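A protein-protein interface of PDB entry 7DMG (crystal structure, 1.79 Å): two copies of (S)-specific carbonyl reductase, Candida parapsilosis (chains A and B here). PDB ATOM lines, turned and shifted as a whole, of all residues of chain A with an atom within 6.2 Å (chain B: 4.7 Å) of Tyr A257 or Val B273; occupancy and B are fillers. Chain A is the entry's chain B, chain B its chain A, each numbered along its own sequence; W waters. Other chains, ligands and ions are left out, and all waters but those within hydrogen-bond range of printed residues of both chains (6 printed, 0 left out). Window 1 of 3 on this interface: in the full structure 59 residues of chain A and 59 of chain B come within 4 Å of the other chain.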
ATOM      1  N   PHE A  31      -3.966 -19.160   5.908  1.00  0.00           N
ATOM      2  CA  PHE A  31      -4.854 -19.643   6.958  1.00  0.00           C
ATOM      3  C   PHE A  31      -6.328 -19.440   6.632  1.00  0.00           C
ATOM      4  O   PHE A  31      -7.185 -19.867   7.416  1.00  0.00           O
ATOM      5  CB  PHE A  31      -4.515 -18.958   8.286  1.00  0.00           C
ATOM      6  CG  PHE A  31      -3.221 -19.432   8.894  1.00  0.00           C
ATOM      7  CD1 PHE A  31      -2.019 -18.823   8.563  1.00  0.00           C
ATOM      8  CD2 PHE A  31      -3.205 -20.499   9.780  1.00  0.00           C
ATOM      9  CE1 PHE A  31      -0.825 -19.259   9.110  1.00  0.00           C
ATOM     10  CE2 PHE A  31      -2.012 -20.944  10.333  1.00  0.00           C
ATOM     11  CZ  PHE A  31      -0.818 -20.326   9.996  1.00  0.00           C
ATOM     12  N   TYR A  55     -13.467 -21.787  12.475  1.00  0.00           N
ATOM     13  CA  TYR A  55     -13.489 -22.040  11.036  1.00  0.00           C
ATOM     14  C   TYR A  55     -14.393 -21.039  10.324  1.00  0.00           C
ATOM     15  O   TYR A  55     -14.087 -20.599   9.206  1.00  0.00           O
ATOM     16  CB  TYR A  55     -13.945 -23.472  10.755  1.00  0.00           C
ATOM     17  CG  TYR A  55     -12.891 -24.529  11.006  1.00  0.00           C
ATOM     18  CD1 TYR A  55     -11.612 -24.191  11.458  1.00  0.00           C
ATOM     19  CD2 TYR A  55     -13.170 -25.867  10.771  1.00  0.00           C
ATOM     20  CE1 TYR A  55     -10.650 -25.169  11.685  1.00  0.00           C
ATOM     21  CE2 TYR A  55     -12.216 -26.846  10.975  1.00  0.00           C
ATOM     22  CZ  TYR A  55     -10.958 -26.498  11.432  1.00  0.00           C
ATOM     23  OH  TYR A  55     -10.024 -27.491  11.640  1.00  0.00           O
ATOM     24  N   ARG A 211      -4.873 -34.734   3.010  1.00  0.00           N
ATOM     25  CA  ARG A 211      -3.982 -34.760   4.155  1.00  0.00           C
ATOM     26  C   ARG A 211      -4.773 -35.198   5.383  1.00  0.00           C
ATOM     27  O   ARG A 211      -5.988 -34.975   5.464  1.00  0.00           O
ATOM     28  CB  ARG A 211      -3.358 -33.381   4.393  1.00  0.00           C
ATOM     29  CG  ARG A 211      -2.464 -32.916   3.238  1.00  0.00           C
ATOM     30  CD  ARG A 211      -1.795 -31.569   3.549  1.00  0.00           C
ATOM     31  NE  ARG A 211      -2.768 -30.479   3.671  1.00  0.00           N
ATOM     32  CZ  ARG A 211      -3.130 -29.905   4.819  1.00  0.00           C
ATOM     33  NH1 ARG A 211      -2.615 -30.318   5.972  1.00  0.00           N
ATOM     34  NH2 ARG A 211      -4.022 -28.920   4.814  1.00  0.00           N
ATOM     35  N   VAL A 252      -7.785 -23.549  18.895  1.00  0.00           N
ATOM     36  CA  VAL A 252      -8.336 -23.290  17.561  1.00  0.00           C
ATOM     37  C   VAL A 252      -7.234 -22.983  16.564  1.00  0.00           C
ATOM     38  O   VAL A 252      -7.390 -23.245  15.363  1.00  0.00           O
ATOM     39  CB  VAL A 252      -9.398 -22.171  17.590  1.00  0.00           C
ATOM     40  CG1 VAL A 252     -10.572 -22.578  18.484  1.00  0.00           C
ATOM     41  CG2 VAL A 252      -8.797 -20.840  18.061  1.00  0.00           C
ATOM     42  N   GLY A 253      -6.106 -22.438  17.022  1.00  0.00           N
ATOM     43  CA  GLY A 253      -5.014 -22.178  16.098  1.00  0.00           C
ATOM     44  C   GLY A 253      -4.487 -23.449  15.461  1.00  0.00           C
ATOM     45  O   GLY A 253      -4.204 -23.483  14.261  1.00  0.00           O
ATOM     46  N   ALA A 254      -4.349 -24.511  16.260  1.00  0.00           N
ATOM     47  CA  ALA A 254      -3.875 -25.791  15.734  1.00  0.00           C
ATOM     48  C   ALA A 254      -4.854 -26.373  14.718  1.00  0.00           C
ATOM     49  O   ALA A 254      -4.447 -26.885  13.661  1.00  0.00           O
ATOM     50  CB  ALA A 254      -3.667 -26.765  16.896  1.00  0.00           C
ATOM     51  N   TYR A 255      -6.150 -26.310  15.020  1.00  0.00           N
ATOM     52  CA  TYR A 255      -7.141 -26.845  14.089  1.00  0.00           C
ATOM     53  C   TYR A 255      -7.214 -26.015  12.809  1.00  0.00           C
ATOM     54  O   TYR A 255      -7.477 -26.555  11.726  1.00  0.00           O
ATOM     55  CB  TYR A 255      -8.516 -26.918  14.760  1.00  0.00           C
ATOM     56  CG  TYR A 255      -8.676 -28.080  15.709  1.00  0.00           C
ATOM     57  CD1 TYR A 255      -9.203 -29.295  15.272  1.00  0.00           C
ATOM     58  CD2 TYR A 255      -8.326 -27.953  17.055  1.00  0.00           C
ATOM     59  CE1 TYR A 255      -9.358 -30.363  16.141  1.00  0.00           C
ATOM     60  CE2 TYR A 255      -8.471 -29.019  17.937  1.00  0.00           C
ATOM     61  CZ  TYR A 255      -8.989 -30.216  17.473  1.00  0.00           C
ATOM     62  OH  TYR A 255      -9.153 -31.268  18.356  1.00  0.00           O
ATOM     63  N   LEU A 256      -7.021 -24.697  12.903  1.00  0.00           N
ATOM     64  CA  LEU A 256      -7.022 -23.895  11.678  1.00  0.00           C
ATOM     65  C   LEU A 256      -5.751 -24.119  10.868  1.00  0.00           C
ATOM     66  O   LEU A 256      -5.796 -24.161   9.632  1.00  0.00           O
ATOM     67  CB  LEU A 256      -7.201 -22.406  12.003  1.00  0.00           C
ATOM     68  CG  LEU A 256      -7.262 -21.482  10.773  1.00  0.00           C
ATOM     69  CD1 LEU A 256      -8.470 -21.813   9.905  1.00  0.00           C
ATOM     70  CD2 LEU A 256      -7.305 -20.011  11.167  1.00  0.00           C
ATOM     71  N   TYR A 257      -4.609 -24.254  11.547  1.00  0.00           N
ATOM     72  CA  TYR A 257      -3.359 -24.567  10.863  1.00  0.00           C
ATOM     73  C   TYR A 257      -3.509 -25.825  10.008  1.00  0.00           C
ATOM     74  O   TYR A 257      -3.209 -25.814   8.809  1.00  0.00           O
ATOM     75  CB  TYR A 257      -2.231 -24.727  11.895  1.00  0.00           C
ATOM     76  CG  TYR A 257      -1.006 -25.381  11.308  1.00  0.00           C
ATOM     77  CD1 TYR A 257      -0.187 -24.677  10.441  1.00  0.00           C
ATOM     78  CD2 TYR A 257      -0.668 -26.699  11.609  1.00  0.00           C
ATOM     79  CE1 TYR A 257       0.937 -25.260   9.871  1.00  0.00           C
ATOM     80  CE2 TYR A 257       0.475 -27.303  11.033  1.00  0.00           C
ATOM     81  CZ  TYR A 257       1.266 -26.568  10.172  1.00  0.00           C
ATOM     82  OH  TYR A 257       2.385 -27.131   9.569  1.00  0.00           O
ATOM     83  N   LEU A 258      -4.015 -26.910  10.604  1.00  0.00           N
ATOM     84  CA  LEU A 258      -4.124 -28.185   9.903  1.00  0.00           C
ATOM     85  C   LEU A 258      -5.222 -28.170   8.843  1.00  0.00           C
ATOM     86  O   LEU A 258      -5.106 -28.863   7.821  1.00  0.00           O
ATOM     87  CB  LEU A 258      -4.372 -29.303  10.921  1.00  0.00           C
ATOM     88  CG  LEU A 258      -3.221 -29.548  11.912  1.00  0.00           C
ATOM     89  CD1 LEU A 258      -3.639 -30.521  13.008  1.00  0.00           C
ATOM     90  CD2 LEU A 258      -1.995 -30.067  11.151  1.00  0.00           C
ATOM     91  N   ALA A 259      -6.285 -27.390   9.053  1.00  0.00           N
ATOM     92  CA  ALA A 259      -7.385 -27.366   8.089  1.00  0.00           C
ATOM     93  C   ALA A 259      -7.038 -26.594   6.824  1.00  0.00           C
ATOM     94  O   ALA A 259      -7.612 -26.866   5.758  1.00  0.00           O
ATOM     95  CB  ALA A 259      -8.636 -26.737   8.713  1.00  0.00           C
ATOM     96  N   SER A 260      -6.127 -25.630   6.919  1.00  0.00           N
ATOM     97  CA  SER A 260      -5.931 -24.629   5.880  1.00  0.00           C
ATOM     98  C   SER A 260      -4.682 -24.927   5.053  1.00  0.00           C
ATOM     99  O   SER A 260      -3.947 -25.887   5.300  1.00  0.00           O
ATOM    100  CB  SER A 260      -5.841 -23.242   6.515  1.00  0.00           C
ATOM    101  OG  SER A 260      -4.628 -23.124   7.249  1.00  0.00           O
ATOM    102  N   ASN A 261      -4.434 -24.065   4.063  1.00  0.00           N
ATOM    103  CA  ASN A 261      -3.261 -24.162   3.203  1.00  0.00           C
ATOM    104  C   ASN A 261      -1.981 -23.778   3.931  1.00  0.00           C
ATOM    105  O   ASN A 261      -0.919 -23.763   3.310  1.00  0.00           O
ATOM    106  CB  ASN A 261      -3.435 -23.268   1.972  1.00  0.00           C
ATOM    107  CG  ASN A 261      -4.200 -23.957   0.833  1.00  0.00           C
ATOM    108  OD1 ASN A 261      -4.602 -25.119   0.936  1.00  0.00           O
ATOM    109  ND2 ASN A 261      -4.438 -23.219  -0.237  1.00  0.00           N
ATOM    110  N   ALA A 262      -2.057 -23.449   5.228  1.00  0.00           N
ATOM    111  CA  ALA A 262      -0.852 -23.215   6.008  1.00  0.00           C
ATOM    112  C   ALA A 262      -0.036 -24.486   6.188  1.00  0.00           C
ATOM    113  O   ALA A 262       1.151 -24.399   6.510  1.00  0.00           O
ATOM    114  CB  ALA A 262      -1.215 -22.633   7.387  1.00  0.00           C
ATOM    115  N   SER A 263      -0.634 -25.658   5.969  1.00  0.00           N
ATOM    116  CA  SER A 263      -0.033 -26.934   6.346  1.00  0.00           C
ATOM    117  C   SER A 263       0.005 -27.916   5.177  1.00  0.00           C
ATOM    118  O   SER A 263      -0.158 -29.124   5.367  1.00  0.00           O
ATOM    119  CB  SER A 263      -0.796 -27.541   7.523  1.00  0.00           C
ATOM    120  OG  SER A 263      -2.160 -27.748   7.176  1.00  0.00           O
ATOM    121  N   THR A 264       0.259 -27.435   3.948  1.00  0.00           N
ATOM    122  CA  THR A 264       0.123 -28.318   2.786  1.00  0.00           C
ATOM    123  C   THR A 264       1.227 -29.374   2.669  1.00  0.00           C
ATOM    124  O   THR A 264       1.079 -30.297   1.859  1.00  0.00           O
ATOM    125  CB  THR A 264       0.075 -27.531   1.467  1.00  0.00           C
ATOM    126  OG1 THR A 264       1.251 -26.724   1.326  1.00  0.00           O
ATOM    127  CG2 THR A 264      -1.164 -26.651   1.410  1.00  0.00           C
ATOM    128  N   TYR A 265       2.312 -29.285   3.441  1.00  0.00           N
ATOM    129  CA  TYR A 265       3.291 -30.366   3.506  1.00  0.00           C
ATOM    130  C   TYR A 265       3.206 -31.132   4.821  1.00  0.00           C
ATOM    131  O   TYR A 265       4.097 -31.933   5.122  1.00  0.00           O
ATOM    132  CB  TYR A 265       4.710 -29.827   3.310  1.00  0.00           C
ATOM    133  CG  TYR A 265       5.733 -30.859   2.861  1.00  0.00           C
ATOM    134  CD1 TYR A 265       5.542 -31.577   1.691  1.00  0.00           C
ATOM    135  CD2 TYR A 265       6.904 -31.095   3.601  1.00  0.00           C
ATOM    136  CE1 TYR A 265       6.471 -32.518   1.261  1.00  0.00           C
ATOM    137  CE2 TYR A 265       7.847 -32.027   3.171  1.00  0.00           C
ATOM    138  CZ  TYR A 265       7.620 -32.733   1.991  1.00  0.00           C
ATOM    139  OH  TYR A 265       8.528 -33.668   1.522  1.00  0.00           O
ATOM    140  N   THR A 266       2.152 -30.904   5.604  1.00  0.00           N
ATOM    141  CA  THR A 266       1.973 -31.519   6.916  1.00  0.00           C
ATOM    142  C   THR A 266       0.920 -32.607   6.788  1.00  0.00           C
ATOM    143  O   THR A 266      -0.240 -32.317   6.489  1.00  0.00           O
ATOM    144  CB  THR A 266       1.549 -30.482   7.955  1.00  0.00           C
ATOM    145  OG1 THR A 266       2.458 -29.367   7.936  1.00  0.00           O
ATOM    146  CG2 THR A 266       1.473 -31.096   9.377  1.00  0.00           C
ATOM    147  N   THR A 267       1.328 -33.854   6.979  1.00  0.00           N
ATOM    148  CA  THR A 267       0.374 -34.946   6.935  1.00  0.00           C
ATOM    149  C   THR A 267       0.909 -36.084   7.793  1.00  0.00           C
ATOM    150  O   THR A 267       2.123 -36.280   7.904  1.00  0.00           O
ATOM    151  CB  THR A 267       0.079 -35.391   5.493  1.00  0.00           C
ATOM    152  OG1 THR A 267      -1.111 -36.186   5.492  1.00  0.00           O
ATOM    153  CG2 THR A 267       1.250 -36.188   4.884  1.00  0.00           C
ATOM    154  N   ALA A 269       0.801 -35.911  10.944  1.00  0.00           N
ATOM    155  CA  ALA A 269       1.387 -35.298  12.128  1.00  0.00           C
ATOM    156  C   ALA A 269       0.397 -35.296  13.282  1.00  0.00           C
ATOM    157  O   ALA A 269      -0.821 -35.227  13.086  1.00  0.00           O
ATOM    158  CB  ALA A 269       1.841 -33.867  11.831  1.00  0.00           C
ATOM    159  N   LEU A 271      -0.210 -32.974  16.535  1.00  0.00           N
ATOM    160  CA  LEU A 271       0.074 -31.703  17.195  1.00  0.00           C
ATOM    161  C   LEU A 271      -0.404 -31.729  18.644  1.00  0.00           C
ATOM    162  O   LEU A 271      -1.601 -31.692  18.932  1.00  0.00           O
ATOM    163  CB  LEU A 271      -0.510 -30.551  16.387  1.00  0.00           C
ATOM    164  CG  LEU A 271      -0.419 -29.149  16.966  1.00  0.00           C
ATOM    165  CD1 LEU A 271       0.971 -28.741  17.334  1.00  0.00           C
ATOM    166  CD2 LEU A 271      -0.753 -28.310  15.733  1.00  0.00           C
ATOM    167  N   VAL B 215      10.135 -27.236  15.199  1.00  0.00           N
ATOM    168  CA  VAL B 215       9.607 -27.689  13.922  1.00  0.00           C
ATOM    169  C   VAL B 215      10.606 -28.687  13.368  1.00  0.00           C
ATOM    170  O   VAL B 215      11.817 -28.429  13.391  1.00  0.00           O
ATOM    171  CB  VAL B 215       9.399 -26.516  12.948  1.00  0.00           C
ATOM    172  CG1 VAL B 215       8.881 -27.004  11.578  1.00  0.00           C
ATOM    173  CG2 VAL B 215       8.444 -25.485  13.536  1.00  0.00           C
ATOM    174  N   SER B 216      10.114 -29.831  12.888  1.00  0.00           N
ATOM    175  CA  SER B 216      10.986 -30.840  12.287  1.00  0.00           C
ATOM    176  C   SER B 216      10.674 -30.976  10.796  1.00  0.00           C
ATOM    177  O   SER B 216       9.849 -31.818  10.394  1.00  0.00           O
ATOM    178  CB  SER B 216      10.838 -32.183  13.009  1.00  0.00           C
ATOM    179  OG  SER B 216      11.452 -32.115  14.307  1.00  0.00           O
ATOM    180  N   PRO B 217      11.285 -30.158   9.936  1.00  0.00           N
ATOM    181  CA  PRO B 217      11.046 -30.297   8.494  1.00  0.00           C
ATOM    182  C   PRO B 217      11.586 -31.606   7.953  1.00  0.00           C
ATOM    183  O   PRO B 217      12.568 -32.157   8.456  1.00  0.00           O
ATOM    184  CB  PRO B 217      11.800 -29.106   7.882  1.00  0.00           C
ATOM    185  CG  PRO B 217      12.104 -28.180   9.065  1.00  0.00           C
ATOM    186  CD  PRO B 217      12.274 -29.108  10.226  1.00  0.00           C
ATOM    187  N   GLY B 218      10.926 -32.096   6.900  1.00  0.00           N
ATOM    188  CA  GLY B 218      11.463 -33.170   6.077  1.00  0.00           C
ATOM    189  C   GLY B 218      12.401 -32.623   5.022  1.00  0.00           C
ATOM    190  O   GLY B 218      13.117 -31.651   5.273  1.00  0.00           O
ATOM    191  N   ILE B 220      13.289 -30.354   2.210  1.00  0.00           N
ATOM    192  CA  ILE B 220      12.800 -29.083   1.683  1.00  0.00           C
ATOM    193  C   ILE B 220      13.676 -28.684   0.508  1.00  0.00           C
ATOM    194  O   ILE B 220      14.905 -28.649   0.626  1.00  0.00           O
ATOM    195  CB  ILE B 220      12.802 -27.979   2.759  1.00  0.00           C
ATOM    196  CG1 ILE B 220      12.136 -28.468   4.044  1.00  0.00           C
ATOM    197  CG2 ILE B 220      12.093 -26.731   2.241  1.00  0.00           C
ATOM    198  CD1 ILE B 220      10.680 -28.866   3.883  1.00  0.00           C
ATOM    199  N   GLU B 250       5.912 -23.853   2.605  1.00  0.00           N
ATOM    200  CA  GLU B 250       5.077 -24.797   3.327  1.00  0.00           C
ATOM    201  C   GLU B 250       5.475 -24.954   4.790  1.00  0.00           C
ATOM    202  O   GLU B 250       4.779 -25.656   5.536  1.00  0.00           O
ATOM    203  CB  GLU B 250       5.102 -26.155   2.615  1.00  0.00           C
ATOM    204  CG  GLU B 250       4.412 -26.117   1.265  1.00  0.00           C
ATOM    205  CD  GLU B 250       4.445 -27.445   0.536  1.00  0.00           C
ATOM    206  OE1 GLU B 250       5.546 -27.945   0.208  1.00  0.00           O
ATOM    207  OE2 GLU B 250       3.341 -28.012   0.341  1.00  0.00           O
ATOM    208  N   LEU B 251       6.557 -24.301   5.227  1.00  0.00           N
ATOM    209  CA  LEU B 251       6.963 -24.308   6.627  1.00  0.00           C
ATOM    210  C   LEU B 251       6.503 -23.088   7.409  1.00  0.00           C
ATOM    211  O   LEU B 251       6.416 -23.166   8.641  1.00  0.00           O
ATOM    212  CB  LEU B 251       8.491 -24.387   6.735  1.00  0.00           C
ATOM    213  CG  LEU B 251       9.193 -25.637   6.221  1.00  0.00           C
ATOM    214  CD1 LEU B 251      10.684 -25.431   6.324  1.00  0.00           C
ATOM    215  CD2 LEU B 251       8.775 -26.835   7.050  1.00  0.00           C
ATOM    216  N   GLY B 253       3.758 -21.470   7.961  1.00  0.00           N
ATOM    217  CA  GLY B 253       2.583 -21.585   8.814  1.00  0.00           C
ATOM    218  C   GLY B 253       2.900 -22.176  10.174  1.00  0.00           C
ATOM    219  O   GLY B 253       2.380 -21.719  11.197  1.00  0.00           O
ATOM    220  N   ALA B 254       3.753 -23.201  10.208  1.00  0.00           N
ATOM    221  CA  ALA B 254       4.111 -23.831  11.476  1.00  0.00           C
ATOM    222  C   ALA B 254       4.910 -22.877  12.354  1.00  0.00           C
ATOM    223  O   ALA B 254       4.699 -22.811  13.574  1.00  0.00           O
ATOM    224  CB  ALA B 254       4.906 -25.115  11.209  1.00  0.00           C
ATOM    225  N   LEU B 271       6.627 -30.226  15.935  1.00  0.00           N
ATOM    226  CA  LEU B 271       5.674 -30.162  14.834  1.00  0.00           C
ATOM    227  C   LEU B 271       6.348 -30.689  13.569  1.00  0.00           C
ATOM    228  O   LEU B 271       7.226 -30.034  13.001  1.00  0.00           O
ATOM    229  CB  LEU B 271       5.153 -28.737  14.689  1.00  0.00           C
ATOM    230  CG  LEU B 271       4.174 -28.389  13.585  1.00  0.00           C
ATOM    231  CD1 LEU B 271       3.124 -29.484  13.468  1.00  0.00           C
ATOM    232  CD2 LEU B 271       3.503 -27.060  14.026  1.00  0.00           C
ATOM    233  N   ALA B 272       5.953 -31.892  13.151  1.00  0.00           N
ATOM    234  CA  ALA B 272       6.552 -32.514  11.976  1.00  0.00           C
ATOM    235  C   ALA B 272       5.950 -31.902  10.721  1.00  0.00           C
ATOM    236  O   ALA B 272       4.726 -31.867  10.564  1.00  0.00           O
ATOM    237  CB  ALA B 272       6.318 -34.026  11.997  1.00  0.00           C
ATOM    238  N   VAL B 273       6.807 -31.415   9.826  1.00  0.00           N
ATOM    239  CA  VAL B 273       6.355 -30.919   8.530  1.00  0.00           C
ATOM    240  C   VAL B 273       7.195 -31.614   7.475  1.00  0.00           C
ATOM    241  O   VAL B 273       8.172 -31.049   6.974  1.00  0.00           O
ATOM    242  CB  VAL B 273       6.469 -29.385   8.424  1.00  0.00           C
ATOM    243  CG1 VAL B 273       5.841 -28.900   7.113  1.00  0.00           C
ATOM    244  CG2 VAL B 273       5.782 -28.710   9.618  1.00  0.00           C
ATOM    245  N   ASP B 274       6.822 -32.851   7.138  1.00  0.00           N
ATOM    246  CA  ASP B 274       7.742 -33.728   6.429  1.00  0.00           C
ATOM    247  C   ASP B 274       7.047 -34.538   5.346  1.00  0.00           C
ATOM    248  O   ASP B 274       7.588 -35.554   4.904  1.00  0.00           O
ATOM    249  CB  ASP B 274       8.444 -34.627   7.463  1.00  0.00           C
ATOM    250  CG  ASP B 274       7.468 -35.509   8.253  1.00  0.00           C
ATOM    251  OD1 ASP B 274       7.888 -36.072   9.280  1.00  0.00           O
ATOM    252  OD2 ASP B 274       6.315 -35.711   7.824  1.00  0.00           O
ATOM    253  N   GLY B 275       5.867 -34.118   4.899  1.00  0.00           N
ATOM    254  CA  GLY B 275       5.215 -34.862   3.832  1.00  0.00           C
ATOM    255  C   GLY B 275       4.811 -36.259   4.245  1.00  0.00           C
ATOM    256  O   GLY B 275       4.557 -37.107   3.384  1.00  0.00           O
HETATM  257  O   HOH W   1       3.041 -27.645   5.689  1.00  0.00           O
HETATM  258  O   HOH W   2      10.110 -35.062   3.405  1.00  0.00           O
HETATM  259  O   HOH W   3       3.556 -25.245   7.983  1.00  0.00           O
HETATM  260  O   HOH W   4       3.147 -22.787   5.530  1.00  0.00           O
HETATM  261  O   HOH W   5       4.184 -33.656   8.471  1.00  0.00           O
HETATM  262  O   HOH W   6       4.454 -36.423   9.725  1.00  0.00           O
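Of the 21 printed residues of chain A, 8 touch a printed residue of chain B.
Along chain A the printed residues that touch a printed residue of chain B span positions 31 to 269.
Of the 14 printed residues of chain B, 7 touch a printed residue of chain A.
Printed residues of chain B that touch a printed residue of chain A: Glu B250, Gly B253, Ala B254, Ala B272, Val B273, Asp B274 and Gly B275.
Among the printed residues, no Asp or Glu carboxylate lies within 4 Å of a Lys or Arg side-chain nitrogen of the other chain.
N of Val B273 is in hydrogen-bond range of O of Ser B216, 3.1 Å away.
N of Gly B218 is in hydrogen-bond range of O of Val B273 (2.9 Å).
NH1 of Arg A211 is in hydrogen-bond range of O of Thr A266 (3.1 Å).
The backbone carbonyl oxygen (O) of Tyr A257 sits at hydrogen-bond distance from the side-chain hydroxyl (OG) of Ser A263.
The side-chain hydroxyl of Tyr A257 lies within hydrogen-bond range of the side-chain hydroxyl of Thr A266, 2.8 Å away.
OG of Ser A260 sits close to N of Ala A262, 3.3 Å away.
Of the printed residues of chain B, Phe A31 touches Gly B253 (3.7 Å).
Printed residues of chain B within 4 Å of Thr A266: Ala B272 (3.5 Å) and Val B273 (3.5 Å).
Pro B217 touches none of the printed residues of chain A.
Printed residues of chain A within 4 Å of Gly B253: Phe A31, Tyr A257 and Ala A262.
Of chain A, only Tyr A257 (3.7 Å), Tyr A265 (3.6 Å) and Thr A266 (3.5 Å) come within 4 Å of Val B273.
The nearest printed residue of chain B that does not touch Phe A31 is Ala B254 (5.4 Å).
OE2 of Glu B250 sits at hydrogen-bond distance from OG1 of Thr A264 (2.6 Å).
The backbone carbonyl oxygen of Tyr A265 sits at hydrogen-bond distance from the backbone NH of Gly B275, 2.8 Å away.
Positions printed for both chains: 253, 254 and 271.
Among the printed residues, merely in contact across the chains: Phe A31 with Gly B253 (3.7 Å), Tyr A257 with Gly B253 (3.7 Å), Tyr A257 with Ala B254 (3.5 Å), Tyr A257 with Val B273 (3.7 Å), Ala A262 with Glu B250 (3.96 Å), Ala A262 with Gly B253 (3.9 Å), Tyr A265 with Glu B250 (3.5 Å), Tyr A265 with Val B273 (3.6 Å), Tyr A265 with Asp B274 (3.4 Å), Thr A266 with Ala B272 (3.5 Å), Thr A266 with Val B273 (3.5 Å), Thr A267 with Gly B275 (3.6 Å) and Ala A269 with Ala B272 (3.7 Å).
Water W1 lies within hydrogen-bond range of the backbone carbonyl oxygen (O) of Glu B250, the backbone NH (N) of Tyr A265, the side-chain hydroxyl (OG1) of Thr A266 and the backbone NH (N) of Thr A264.
Water W3 lies within hydrogen-bond range of OH of Tyr A257 (2.7 Å), O of Glu B250 (2.8 Å), O of Ala A262 (2.9 Å) and N of Ala B254 (3.0 Å).
Water W4 lies within hydrogen-bond range of O of Ala A262, N of Gly B253 and O of Glu B250.
Water W6 lies within hydrogen-bond range of OD2 of Asp B274 (2.8 Å) and O of Thr A267 (3.0 Å).
Water W5 lies within hydrogen-bond range of O of Ala B272 (2.8 Å), OD2 of Asp B274 (3.0 Å) and N of Thr A267 (3.2 Å).
Water W2 lies within hydrogen-bond range of the side-chain hydroxyl (OH) of Tyr A265 (2.8 Å) and the backbone carbonyl oxygen (O) of Asp B274 (3.0 Å).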
